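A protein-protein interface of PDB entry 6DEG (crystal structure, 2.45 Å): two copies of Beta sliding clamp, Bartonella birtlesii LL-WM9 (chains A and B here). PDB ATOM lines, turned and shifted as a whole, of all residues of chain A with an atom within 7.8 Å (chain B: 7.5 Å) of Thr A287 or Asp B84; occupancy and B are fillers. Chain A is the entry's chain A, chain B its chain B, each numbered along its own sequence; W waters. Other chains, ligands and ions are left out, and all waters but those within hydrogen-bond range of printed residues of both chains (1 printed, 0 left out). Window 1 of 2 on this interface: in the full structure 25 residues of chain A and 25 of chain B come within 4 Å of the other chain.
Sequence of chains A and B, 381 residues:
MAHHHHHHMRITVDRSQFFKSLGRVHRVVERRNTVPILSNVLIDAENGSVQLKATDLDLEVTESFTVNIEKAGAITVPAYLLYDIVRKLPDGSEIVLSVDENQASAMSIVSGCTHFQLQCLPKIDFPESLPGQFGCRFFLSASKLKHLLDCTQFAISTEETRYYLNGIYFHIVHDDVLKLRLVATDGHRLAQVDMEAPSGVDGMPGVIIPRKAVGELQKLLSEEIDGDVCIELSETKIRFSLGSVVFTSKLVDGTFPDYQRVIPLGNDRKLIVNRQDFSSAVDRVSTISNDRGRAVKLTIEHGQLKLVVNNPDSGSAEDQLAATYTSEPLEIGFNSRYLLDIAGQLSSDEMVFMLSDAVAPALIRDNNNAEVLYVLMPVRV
No position is printed for both chains. Of the 12 pairs that touch across the chains among the printed residues, none has its exchanged pair printed and touching as well.
The backbone NH (N) of Ala A317 lies within hydrogen-bond range of the backbone carbonyl oxygen (O) of Val A309, 2.8 Å away. O of Arg A284 sits at hydrogen-bond distance from OG1 of Thr A287 (3.0 Å). The backbone carbonyl oxygen of Ile A288 is in hydrogen-bond range of the side-chain amide nitrogen of Asn A311 (2.8 Å). The backbone carbonyl oxygen (O) of Asp A283 lies within hydrogen-bond range of the side-chain hydroxyl (OG) of Ser A286 (3.2 Å). The backbone carbonyl oxygen (O) of Leu B89 lies within hydrogen-bond range of the guanidinium group (NE) of Arg B15 (2.9 Å). OD1 of Asp B84 is in salt-bridge range of NH1 of Arg B87 (2.8 Å).
Thr A287 touches just these residues of chain B: Leu B81 (3.2 Å), Asp B84 (3.5 Å), Ile B85 (3.6 Å) and Lys B88 (3.3 Å). Of chain A, only Thr A287 (3.5 Å) comes within 4 Å of Asp B84. Printed residues of chain A within 4 Å of Leu B89: Arg A284. Printed residues of chain B within 4 Å of Asp A283: Lys B88. Of the printed residues of chain B, Arg A284 touches Lys B88 (3.7 Å), Leu B89 (3.7 Å) and Phe B116 (3.4 Å). Printed residues of chain B within 4 Å of Ile A288: Leu B81, Ile B85 and Phe B116.
Water W1 bridges the side-chain amide nitrogen (ND2) of Asn A290 (2.9 Å) and the side-chain amino group (NZ) of Lys B88 (2.9 Å).
Among the printed residues, merely in contact across the chains: Arg A284 with Lys B88, Arg A284 with Leu B89, Arg A284 with Phe B116, Thr A287 with Leu B81, Thr A287 with Asp B84, Thr A287 with Ile B85, Ile A288 with Leu B81, Ile A288 with Ile B85, Ile A288 with Phe B116 and Ala A317 with Phe B116.
OD1 of Asp A283 is in salt-bridge range of NZ of Lys B88 (3.7 Å). NZ of Lys B88 sits at hydrogen-bond distance from OG1 of Thr A287 (3.3 Å).
Of the 16 printed residues of chain B, 6 touch a printed residue of chain A. Printed residues of chain A that touch a printed residue of chain B: Asp A283, Arg A284, Thr A287, Ile A288 and Ala A317. Hydrophobic or aromatic side chains of chain A that line the printed part of chain B: Ile A288 and Ala A317. Among the printed residues, Asp or Glu carboxylates within 4 Å of a Lys or Arg side-chain nitrogen of the other chain: Asp A283 with Lys B88.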
ATOM      1  N   ALA A 281      20.925 -20.114 -23.309  1.00  0.00           N
ATOM      2  CA  ALA A 281      20.412 -20.590 -24.590  1.00  0.00           C
ATOM      3  C   ALA A 281      20.602 -22.095 -24.742  1.00  0.00           C
ATOM      4  O   ALA A 281      19.698 -22.799 -25.206  1.00  0.00           O
ATOM      5  CB  ALA A 281      21.096 -19.845 -25.735  1.00  0.00           C
ATOM      6  N   VAL A 282      21.773 -22.605 -24.362  1.00  0.00           N
ATOM      7  CA  VAL A 282      22.008 -24.046 -24.406  1.00  0.00           C
ATOM      8  C   VAL A 282      21.063 -24.767 -23.454  1.00  0.00           C
ATOM      9  O   VAL A 282      20.585 -25.872 -23.742  1.00  0.00           O
ATOM     10  CB  VAL A 282      23.481 -24.350 -24.079  1.00  0.00           C
ATOM     11  CG1 VAL A 282      23.698 -25.847 -23.923  1.00  0.00           C
ATOM     12  CG2 VAL A 282      24.386 -23.783 -25.155  1.00  0.00           C
ATOM     13  N   ASP A 283      20.776 -24.147 -22.306  1.00  0.00           N
ATOM     14  CA  ASP A 283      19.884 -24.746 -21.318  1.00  0.00           C
ATOM     15  C   ASP A 283      18.495 -24.986 -21.893  1.00  0.00           C
ATOM     16  O   ASP A 283      17.864 -26.013 -21.610  1.00  0.00           O
ATOM     17  CB  ASP A 283      19.797 -23.837 -20.092  1.00  0.00           C
ATOM     18  CG  ASP A 283      19.762 -24.606 -18.793  1.00  0.00           C
ATOM     19  OD1 ASP A 283      19.678 -25.850 -18.839  1.00  0.00           O
ATOM     20  OD2 ASP A 283      19.818 -23.963 -17.724  1.00  0.00           O
ATOM     21  N   ARG A 284      18.002 -24.047 -22.697  1.00  0.00           N
ATOM     22  CA  ARG A 284      16.614 -24.094 -23.142  1.00  0.00           C
ATOM     23  C   ARG A 284      16.385 -25.163 -24.209  1.00  0.00           C
ATOM     24  O   ARG A 284      15.420 -25.933 -24.125  1.00  0.00           O
ATOM     25  CB  ARG A 284      16.202 -22.707 -23.634  1.00  0.00           C
ATOM     26  CG  ARG A 284      16.250 -21.662 -22.520  1.00  0.00           C
ATOM     27  CD  ARG A 284      15.914 -20.254 -22.991  1.00  0.00           C
ATOM     28  NE  ARG A 284      15.887 -19.308 -21.875  1.00  0.00           N
ATOM     29  CZ  ARG A 284      16.779 -18.340 -21.684  1.00  0.00           C
ATOM     30  NH1 ARG A 284      17.777 -18.173 -22.541  1.00  0.00           N
ATOM     31  NH2 ARG A 284      16.670 -17.534 -20.636  1.00  0.00           N
ATOM     32  N   VAL A 285      17.264 -25.239 -25.213  1.00  0.00           N
ATOM     33  CA  VAL A 285      17.027 -26.138 -26.344  1.00  0.00           C
ATOM     34  C   VAL A 285      17.253 -27.610 -26.013  1.00  0.00           C
ATOM     35  O   VAL A 285      16.697 -28.479 -26.695  1.00  0.00           O
ATOM     36  CB  VAL A 285      17.900 -25.740 -27.552  1.00  0.00           C
ATOM     37  CG1 VAL A 285      17.399 -24.454 -28.178  1.00  0.00           C
ATOM     38  CG2 VAL A 285      19.358 -25.596 -27.136  1.00  0.00           C
ATOM     39  N   SER A 286      18.044 -27.926 -24.992  1.00  0.00           N
ATOM     40  CA  SER A 286      18.319 -29.323 -24.678  1.00  0.00           C
ATOM     41  C   SER A 286      17.174 -30.013 -23.947  1.00  0.00           C
ATOM     42  O   SER A 286      17.271 -31.218 -23.685  1.00  0.00           O
ATOM     43  CB  SER A 286      19.592 -29.425 -23.839  1.00  0.00           C
ATOM     44  OG  SER A 286      19.529 -28.562 -22.721  1.00  0.00           O
ATOM     45  N   THR A 287      16.107 -29.290 -23.606  1.00  0.00           N
ATOM     46  CA  THR A 287      14.970 -29.906 -22.933  1.00  0.00           C
ATOM     47  C   THR A 287      14.175 -30.835 -23.840  1.00  0.00           C
ATOM     48  O   THR A 287      13.533 -31.763 -23.338  1.00  0.00           O
ATOM     49  CB  THR A 287      14.050 -28.827 -22.366  1.00  0.00           C
ATOM     50  OG1 THR A 287      14.840 -27.764 -21.821  1.00  0.00           O
ATOM     51  CG2 THR A 287      13.171 -29.402 -21.274  1.00  0.00           C
ATOM     52  N   ILE A 288      14.220 -30.636 -25.159  1.00  0.00           N
ATOM     53  CA  ILE A 288      13.464 -31.495 -26.067  1.00  0.00           C
ATOM     54  C   ILE A 288      14.251 -32.764 -26.342  1.00  0.00           C
ATOM     55  O   ILE A 288      13.958 -33.500 -27.290  1.00  0.00           O
ATOM     56  CB  ILE A 288      13.105 -30.789 -27.386  1.00  0.00           C
ATOM     57  CG1 ILE A 288      14.356 -30.536 -28.223  1.00  0.00           C
ATOM     58  CG2 ILE A 288      12.316 -29.527 -27.115  1.00  0.00           C
ATOM     59  CD1 ILE A 288      14.700 -31.690 -29.129  1.00  0.00           C
ATOM     60  N   SER A 289      15.260 -33.025 -25.517  1.00  0.00           N
ATOM     61  CA  SER A 289      15.860 -34.338 -25.498  1.00  0.00           C
ATOM     62  C   SER A 289      16.522 -34.498 -24.128  1.00  0.00           C
ATOM     63  O   SER A 289      17.743 -34.519 -23.980  1.00  0.00           O
ATOM     64  CB  SER A 289      16.847 -34.547 -26.649  1.00  0.00           C
ATOM     65  OG  SER A 289      17.072 -35.932 -26.833  1.00  0.00           O
ATOM     66  N   ASN A 290      15.676 -34.608 -23.100  1.00  0.00           N
ATOM     67  CA  ASN A 290      16.125 -35.003 -21.772  1.00  0.00           C
ATOM     68  C   ASN A 290      16.860 -36.339 -21.791  1.00  0.00           C
ATOM     69  O   ASN A 290      17.610 -36.641 -20.856  1.00  0.00           O
ATOM     70  CB  ASN A 290      14.914 -35.071 -20.837  1.00  0.00           C
ATOM     71  CG  ASN A 290      15.287 -34.911 -19.387  1.00  0.00           C
ATOM     72  OD1 ASN A 290      15.480 -35.895 -18.674  1.00  0.00           O
ATOM     73  ND2 ASN A 290      15.382 -33.666 -18.934  1.00  0.00           N
ATOM     74  N   ASP A 291      16.670 -37.132 -22.846  1.00  0.00           N
ATOM     75  CA  ASP A 291      17.243 -38.467 -22.956  1.00  0.00           C
ATOM     76  C   ASP A 291      18.581 -38.436 -23.684  1.00  0.00           C
ATOM     77  O   ASP A 291      19.394 -37.540 -23.450  1.00  0.00           O
ATOM     78  CB  ASP A 291      16.267 -39.395 -23.680  1.00  0.00           C
ATOM     79  CG  ASP A 291      15.561 -38.705 -24.832  1.00  0.00           C
ATOM     80  OD1 ASP A 291      15.791 -37.493 -25.022  1.00  0.00           O
ATOM     81  OD2 ASP A 291      14.774 -39.364 -25.541  1.00  0.00           O
ATOM     82  N   GLY A 293      19.431 -37.858 -26.778  1.00  0.00           N
ATOM     83  CA  GLY A 293      19.693 -36.831 -27.766  1.00  0.00           C
ATOM     84  C   GLY A 293      20.207 -35.544 -27.150  1.00  0.00           C
ATOM     85  O   GLY A 293      19.860 -34.443 -27.591  1.00  0.00           O
ATOM     86  N   VAL A 309      18.504 -28.362 -31.728  1.00  0.00           N
ATOM     87  CA  VAL A 309      18.311 -29.698 -31.180  1.00  0.00           C
ATOM     88  C   VAL A 309      17.091 -30.301 -31.855  1.00  0.00           C
ATOM     89  O   VAL A 309      16.059 -29.636 -32.003  1.00  0.00           O
ATOM     90  CB  VAL A 309      18.147 -29.696 -29.647  1.00  0.00           C
ATOM     91  CG1 VAL A 309      18.287 -31.110 -29.103  1.00  0.00           C
ATOM     92  CG2 VAL A 309      19.171 -28.782 -29.022  1.00  0.00           C
ATOM     93  N   ASN A 311      14.584 -33.980 -32.238  1.00  0.00           N
ATOM     94  CA  ASN A 311      14.138 -35.218 -31.625  1.00  0.00           C
ATOM     95  C   ASN A 311      12.941 -35.741 -32.404  1.00  0.00           C
ATOM     96  O   ASN A 311      11.858 -35.144 -32.347  1.00  0.00           O
ATOM     97  CB  ASN A 311      13.781 -34.988 -30.158  1.00  0.00           C
ATOM     98  CG  ASN A 311      13.716 -36.275 -29.367  1.00  0.00           C
ATOM     99  OD1 ASN A 311      13.429 -37.340 -29.913  1.00  0.00           O
ATOM    100  ND2 ASN A 311      13.976 -36.184 -28.070  1.00  0.00           N
ATOM    101  N   SER A 314      10.035 -36.131 -30.217  1.00  0.00           N
ATOM    102  CA  SER A 314       9.649 -34.953 -29.452  1.00  0.00           C
ATOM    103  C   SER A 314       9.503 -33.706 -30.309  1.00  0.00           C
ATOM    104  O   SER A 314       8.613 -32.895 -30.052  1.00  0.00           O
ATOM    105  CB  SER A 314      10.672 -34.692 -28.338  1.00  0.00           C
ATOM    106  OG  SER A 314      10.702 -35.758 -27.405  1.00  0.00           O
ATOM    107  N   ALA A 317      13.936 -27.775 -31.769  1.00  0.00           N
ATOM    108  CA  ALA A 317      14.134 -26.535 -31.038  1.00  0.00           C
ATOM    109  C   ALA A 317      15.101 -25.643 -31.804  1.00  0.00           C
ATOM    110  O   ALA A 317      15.910 -26.111 -32.609  1.00  0.00           O
ATOM    111  CB  ALA A 317      14.661 -26.788 -29.621  1.00  0.00           C
ATOM    112  N   SER A 336      25.176 -31.532 -24.549  1.00  0.00           N
ATOM    113  CA  SER A 336      24.579 -30.359 -23.915  1.00  0.00           C
ATOM    114  C   SER A 336      25.095 -30.157 -22.495  1.00  0.00           C
ATOM    115  O   SER A 336      25.433 -29.035 -22.106  1.00  0.00           O
ATOM    116  CB  SER A 336      23.058 -30.477 -23.916  1.00  0.00           C
ATOM    117  OG  SER A 336      22.570 -30.707 -25.224  1.00  0.00           O
ATOM    118  N   ARG B  15       4.710 -16.323 -18.552  1.00  0.00           N
ATOM    119  CA  ARG B  15       5.407 -17.587 -18.333  1.00  0.00           C
ATOM    120  C   ARG B  15       5.197 -18.097 -16.914  1.00  0.00           C
ATOM    121  O   ARG B  15       4.825 -19.257 -16.710  1.00  0.00           O
ATOM    122  CB  ARG B  15       6.896 -17.417 -18.633  1.00  0.00           C
ATOM    123  CG  ARG B  15       7.757 -18.603 -18.238  1.00  0.00           C
ATOM    124  CD  ARG B  15       8.524 -18.307 -16.966  1.00  0.00           C
ATOM    125  NE  ARG B  15       9.201 -19.487 -16.444  1.00  0.00           N
ATOM    126  CZ  ARG B  15       9.278 -19.782 -15.153  1.00  0.00           C
ATOM    127  NH1 ARG B  15       9.917 -20.873 -14.756  1.00  0.00           N
ATOM    128  NH2 ARG B  15       8.710 -18.988 -14.257  1.00  0.00           N
ATOM    129  N   PHE B  19       3.546 -21.263 -15.749  1.00  0.00           N
ATOM    130  CA  PHE B  19       4.266 -22.298 -15.020  1.00  0.00           C
ATOM    131  C   PHE B  19       3.506 -22.714 -13.768  1.00  0.00           C
ATOM    132  O   PHE B  19       3.444 -23.904 -13.436  1.00  0.00           O
ATOM    133  CB  PHE B  19       5.659 -21.796 -14.653  1.00  0.00           C
ATOM    134  CG  PHE B  19       6.525 -22.833 -14.015  1.00  0.00           C
ATOM    135  CD1 PHE B  19       6.827 -24.005 -14.682  1.00  0.00           C
ATOM    136  CD2 PHE B  19       7.041 -22.636 -12.748  1.00  0.00           C
ATOM    137  CE1 PHE B  19       7.632 -24.958 -14.102  1.00  0.00           C
ATOM    138  CE2 PHE B  19       7.845 -23.587 -12.159  1.00  0.00           C
ATOM    139  CZ  PHE B  19       8.141 -24.752 -12.838  1.00  0.00           C
ATOM    140  N   LEU B  22       0.632 -24.723 -14.669  1.00  0.00           N
ATOM    141  CA  LEU B  22       1.047 -25.998 -15.231  1.00  0.00           C
ATOM    142  C   LEU B  22       1.470 -26.999 -14.170  1.00  0.00           C
ATOM    143  O   LEU B  22       1.367 -28.208 -14.397  1.00  0.00           O
ATOM    144  CB  LEU B  22       2.200 -25.776 -16.209  1.00  0.00           C
ATOM    145  CG  LEU B  22       2.311 -26.772 -17.354  1.00  0.00           C
ATOM    146  CD1 LEU B  22       1.067 -26.704 -18.211  1.00  0.00           C
ATOM    147  CD2 LEU B  22       3.551 -26.471 -18.175  1.00  0.00           C
ATOM    148  N   HIS B  26       0.346 -30.945 -13.518  1.00  0.00           N
ATOM    149  CA  HIS B  26       1.579 -31.637 -13.874  1.00  0.00           C
ATOM    150  C   HIS B  26       1.605 -33.067 -13.348  1.00  0.00           C
ATOM    151  O   HIS B  26       1.994 -33.995 -14.067  1.00  0.00           O
ATOM    152  CB  HIS B  26       2.766 -30.837 -13.340  1.00  0.00           C
ATOM    153  CG  HIS B  26       4.075 -31.539 -13.468  1.00  0.00           C
ATOM    154  ND1 HIS B  26       5.021 -31.535 -12.467  1.00  0.00           N
ATOM    155  CD2 HIS B  26       4.601 -32.267 -14.482  1.00  0.00           C
ATOM    156  CE1 HIS B  26       6.074 -32.231 -12.857  1.00  0.00           C
ATOM    157  NE2 HIS B  26       5.844 -32.685 -14.077  1.00  0.00           N
ATOM    158  N   ALA B  79       3.406 -33.403 -21.505  1.00  0.00           N
ATOM    159  CA  ALA B  79       3.348 -32.577 -20.302  1.00  0.00           C
ATOM    160  C   ALA B  79       4.710 -32.346 -19.647  1.00  0.00           C
ATOM    161  O   ALA B  79       5.089 -31.197 -19.395  1.00  0.00           O
ATOM    162  CB  ALA B  79       2.390 -33.212 -19.290  1.00  0.00           C
ATOM    163  N   TYR B  80       5.441 -33.416 -19.333  1.00  0.00           N
ATOM    164  CA  TYR B  80       6.725 -33.251 -18.657  1.00  0.00           C
ATOM    165  C   TYR B  80       7.707 -32.475 -19.521  1.00  0.00           C
ATOM    166  O   TYR B  80       8.454 -31.629 -19.017  1.00  0.00           O
ATOM    167  CB  TYR B  80       7.305 -34.611 -18.285  1.00  0.00           C
ATOM    168  CG  TYR B  80       7.034 -34.990 -16.857  1.00  0.00           C
ATOM    169  CD1 TYR B  80       5.791 -35.474 -16.475  1.00  0.00           C
ATOM    170  CD2 TYR B  80       8.015 -34.855 -15.886  1.00  0.00           C
ATOM    171  CE1 TYR B  80       5.535 -35.819 -15.171  1.00  0.00           C
ATOM    172  CE2 TYR B  80       7.769 -35.199 -14.577  1.00  0.00           C
ATOM    173  CZ  TYR B  80       6.527 -35.681 -14.224  1.00  0.00           C
ATOM    174  OH  TYR B  80       6.274 -36.024 -12.918  1.00  0.00           O
ATOM    175  N   LEU B  81       7.717 -32.751 -20.826  1.00  0.00           N
ATOM    176  CA  LEU B  81       8.544 -31.976 -21.741  1.00  0.00           C
ATOM    177  C   LEU B  81       8.201 -30.496 -21.653  1.00  0.00           C
ATOM    178  O   LEU B  81       9.091 -29.641 -21.564  1.00  0.00           O
ATOM    179  CB  LEU B  81       8.362 -32.494 -23.170  1.00  0.00           C
ATOM    180  CG  LEU B  81       8.987 -31.687 -24.310  1.00  0.00           C
ATOM    181  CD1 LEU B  81      10.484 -31.594 -24.131  1.00  0.00           C
ATOM    182  CD2 LEU B  81       8.647 -32.304 -25.657  1.00  0.00           C
ATOM    183  N   LEU B  82       6.906 -30.179 -21.649  1.00  0.00           N
ATOM    184  CA  LEU B  82       6.476 -28.787 -21.600  1.00  0.00           C
ATOM    185  C   LEU B  82       6.708 -28.175 -20.223  1.00  0.00           C
ATOM    186  O   LEU B  82       7.133 -27.018 -20.118  1.00  0.00           O
ATOM    187  CB  LEU B  82       5.005 -28.688 -21.989  1.00  0.00           C
ATOM    188  CG  LEU B  82       4.316 -27.354 -21.730  1.00  0.00           C
ATOM    189  CD1 LEU B  82       4.967 -26.257 -22.546  1.00  0.00           C
ATOM    190  CD2 LEU B  82       2.835 -27.457 -22.053  1.00  0.00           C
ATOM    191  N   TYR B  83       6.426 -28.926 -19.155  1.00  0.00           N
ATOM    192  CA  TYR B  83       6.725 -28.425 -17.818  1.00  0.00           C
ATOM    193  C   TYR B  83       8.211 -28.130 -17.662  1.00  0.00           C
ATOM    194  O   TYR B  83       8.589 -27.074 -17.138  1.00  0.00           O
ATOM    195  CB  TYR B  83       6.264 -29.425 -16.763  1.00  0.00           C
ATOM    196  CG  TYR B  83       6.479 -28.936 -15.351  1.00  0.00           C
ATOM    197  CD1 TYR B  83       5.580 -28.061 -14.756  1.00  0.00           C
ATOM    198  CD2 TYR B  83       7.582 -29.344 -14.613  1.00  0.00           C
ATOM    199  CE1 TYR B  83       5.767 -27.611 -13.465  1.00  0.00           C
ATOM    200  CE2 TYR B  83       7.780 -28.898 -13.321  1.00  0.00           C
ATOM    201  CZ  TYR B  83       6.869 -28.030 -12.751  1.00  0.00           C
ATOM    202  OH  TYR B  83       7.059 -27.581 -11.464  1.00  0.00           O
ATOM    203  N   ASP B  84       9.071 -29.040 -18.127  1.00  0.00           N
ATOM    204  CA  ASP B  84      10.508 -28.822 -18.016  1.00  0.00           C
ATOM    205  C   ASP B  84      10.961 -27.657 -18.886  1.00  0.00           C
ATOM    206  O   ASP B  84      11.929 -26.970 -18.542  1.00  0.00           O
ATOM    207  CB  ASP B  84      11.271 -30.095 -18.388  1.00  0.00           C
ATOM    208  CG  ASP B  84      10.986 -31.246 -17.441  1.00  0.00           C
ATOM    209  OD1 ASP B  84      10.718 -30.988 -16.249  1.00  0.00           O
ATOM    210  OD2 ASP B  84      11.030 -32.412 -17.890  1.00  0.00           O
ATOM    211  N   ILE B  85      10.281 -27.430 -20.011  1.00  0.00           N
ATOM    212  CA  ILE B  85      10.632 -26.321 -20.894  1.00  0.00           C
ATOM    213  C   ILE B  85      10.271 -24.984 -20.253  1.00  0.00           C
ATOM    214  O   ILE B  85      11.093 -24.062 -20.201  1.00  0.00           O
ATOM    215  CB  ILE B  85       9.949 -26.490 -22.264  1.00  0.00           C
ATOM    216  CG1 ILE B  85      10.732 -27.461 -23.148  1.00  0.00           C
ATOM    217  CG2 ILE B  85       9.800 -25.147 -22.962  1.00  0.00           C
ATOM    218  CD1 ILE B  85      10.094 -27.692 -24.502  1.00  0.00           C
ATOM    219  N   VAL B  86       9.035 -24.857 -19.756  1.00  0.00           N
ATOM    220  CA  VAL B  86       8.578 -23.581 -19.208  1.00  0.00           C
ATOM    221  C   VAL B  86       9.338 -23.218 -17.939  1.00  0.00           C
ATOM    222  O   VAL B  86       9.562 -22.033 -17.660  1.00  0.00           O
ATOM    223  CB  VAL B  86       7.058 -23.626 -18.959  1.00  0.00           C
ATOM    224  CG1 VAL B  86       6.570 -22.328 -18.334  1.00  0.00           C
ATOM    225  CG2 VAL B  86       6.322 -23.877 -20.254  1.00  0.00           C
ATOM    226  N   ARG B  87       9.750 -24.217 -17.153  1.00  0.00           N
ATOM    227  CA  ARG B  87      10.568 -23.952 -15.974  1.00  0.00           C
ATOM    228  C   ARG B  87      11.831 -23.173 -16.330  1.00  0.00           C
ATOM    229  O   ARG B  87      12.222 -22.247 -15.611  1.00  0.00           O
ATOM    230  CB  ARG B  87      10.921 -25.262 -15.267  1.00  0.00           C
ATOM    231  CG  ARG B  87      11.715 -25.074 -13.986  1.00  0.00           C
ATOM    232  CD  ARG B  87      12.187 -26.403 -13.437  1.00  0.00           C
ATOM    233  NE  ARG B  87      13.188 -26.997 -14.314  1.00  0.00           N
ATOM    234  CZ  ARG B  87      12.991 -28.104 -15.019  1.00  0.00           C
ATOM    235  NH1 ARG B  87      11.836 -28.750 -14.928  1.00  0.00           N
ATOM    236  NH2 ARG B  87      13.953 -28.573 -15.802  1.00  0.00           N
ATOM    237  N   LYS B  88      12.477 -23.527 -17.443  1.00  0.00           N
ATOM    238  CA  LYS B  88      13.759 -22.941 -17.814  1.00  0.00           C
ATOM    239  C   LYS B  88      13.633 -21.630 -18.581  1.00  0.00           C
ATOM    240  O   LYS B  88      14.638 -20.927 -18.737  1.00  0.00           O
ATOM    241  CB  LYS B  88      14.560 -23.939 -18.655  1.00  0.00           C
ATOM    242  CG  LYS B  88      14.947 -25.200 -17.910  1.00  0.00           C
ATOM    243  CD  LYS B  88      15.282 -26.322 -18.873  1.00  0.00           C
ATOM    244  CE  LYS B  88      16.687 -26.843 -18.658  1.00  0.00           C
ATOM    245  NZ  LYS B  88      16.853 -28.204 -19.245  1.00  0.00           N
ATOM    246  N   LEU B  89      12.445 -21.281 -19.063  1.00  0.00           N
ATOM    247  CA  LEU B  89      12.276 -20.012 -19.756  1.00  0.00           C
ATOM    248  C   LEU B  89      12.307 -18.859 -18.755  1.00  0.00           C
ATOM    249  O   LEU B  89      11.816 -19.001 -17.632  1.00  0.00           O
ATOM    250  CB  LEU B  89      10.970 -19.989 -20.543  1.00  0.00           C
ATOM    251  CG  LEU B  89      11.055 -20.663 -21.911  1.00  0.00           C
ATOM    252  CD1 LEU B  89       9.756 -20.486 -22.676  1.00  0.00           C
ATOM    253  CD2 LEU B  89      12.236 -20.125 -22.706  1.00  0.00           C
ATOM    254  N   PHE B 116      10.370 -23.498 -30.603  1.00  0.00           N
ATOM    255  CA  PHE B 116      10.144 -24.932 -30.507  1.00  0.00           C
ATOM    256  C   PHE B 116       9.077 -25.365 -31.503  1.00  0.00           C
ATOM    257  O   PHE B 116       8.321 -24.550 -32.039  1.00  0.00           O
ATOM    258  CB  PHE B 116       9.708 -25.344 -29.095  1.00  0.00           C
ATOM    259  CG  PHE B 116      10.801 -25.280 -28.065  1.00  0.00           C
ATOM    260  CD1 PHE B 116      11.078 -24.101 -27.397  1.00  0.00           C
ATOM    261  CD2 PHE B 116      11.542 -26.407 -27.755  1.00  0.00           C
ATOM    262  CE1 PHE B 116      12.083 -24.044 -26.443  1.00  0.00           C
ATOM    263  CE2 PHE B 116      12.548 -26.356 -26.802  1.00  0.00           C
ATOM    264  CZ  PHE B 116      12.818 -25.173 -26.147  1.00  0.00           C
HETATM  265  O   HOH W   1      15.652 -30.829 -19.082  1.00  0.00           O
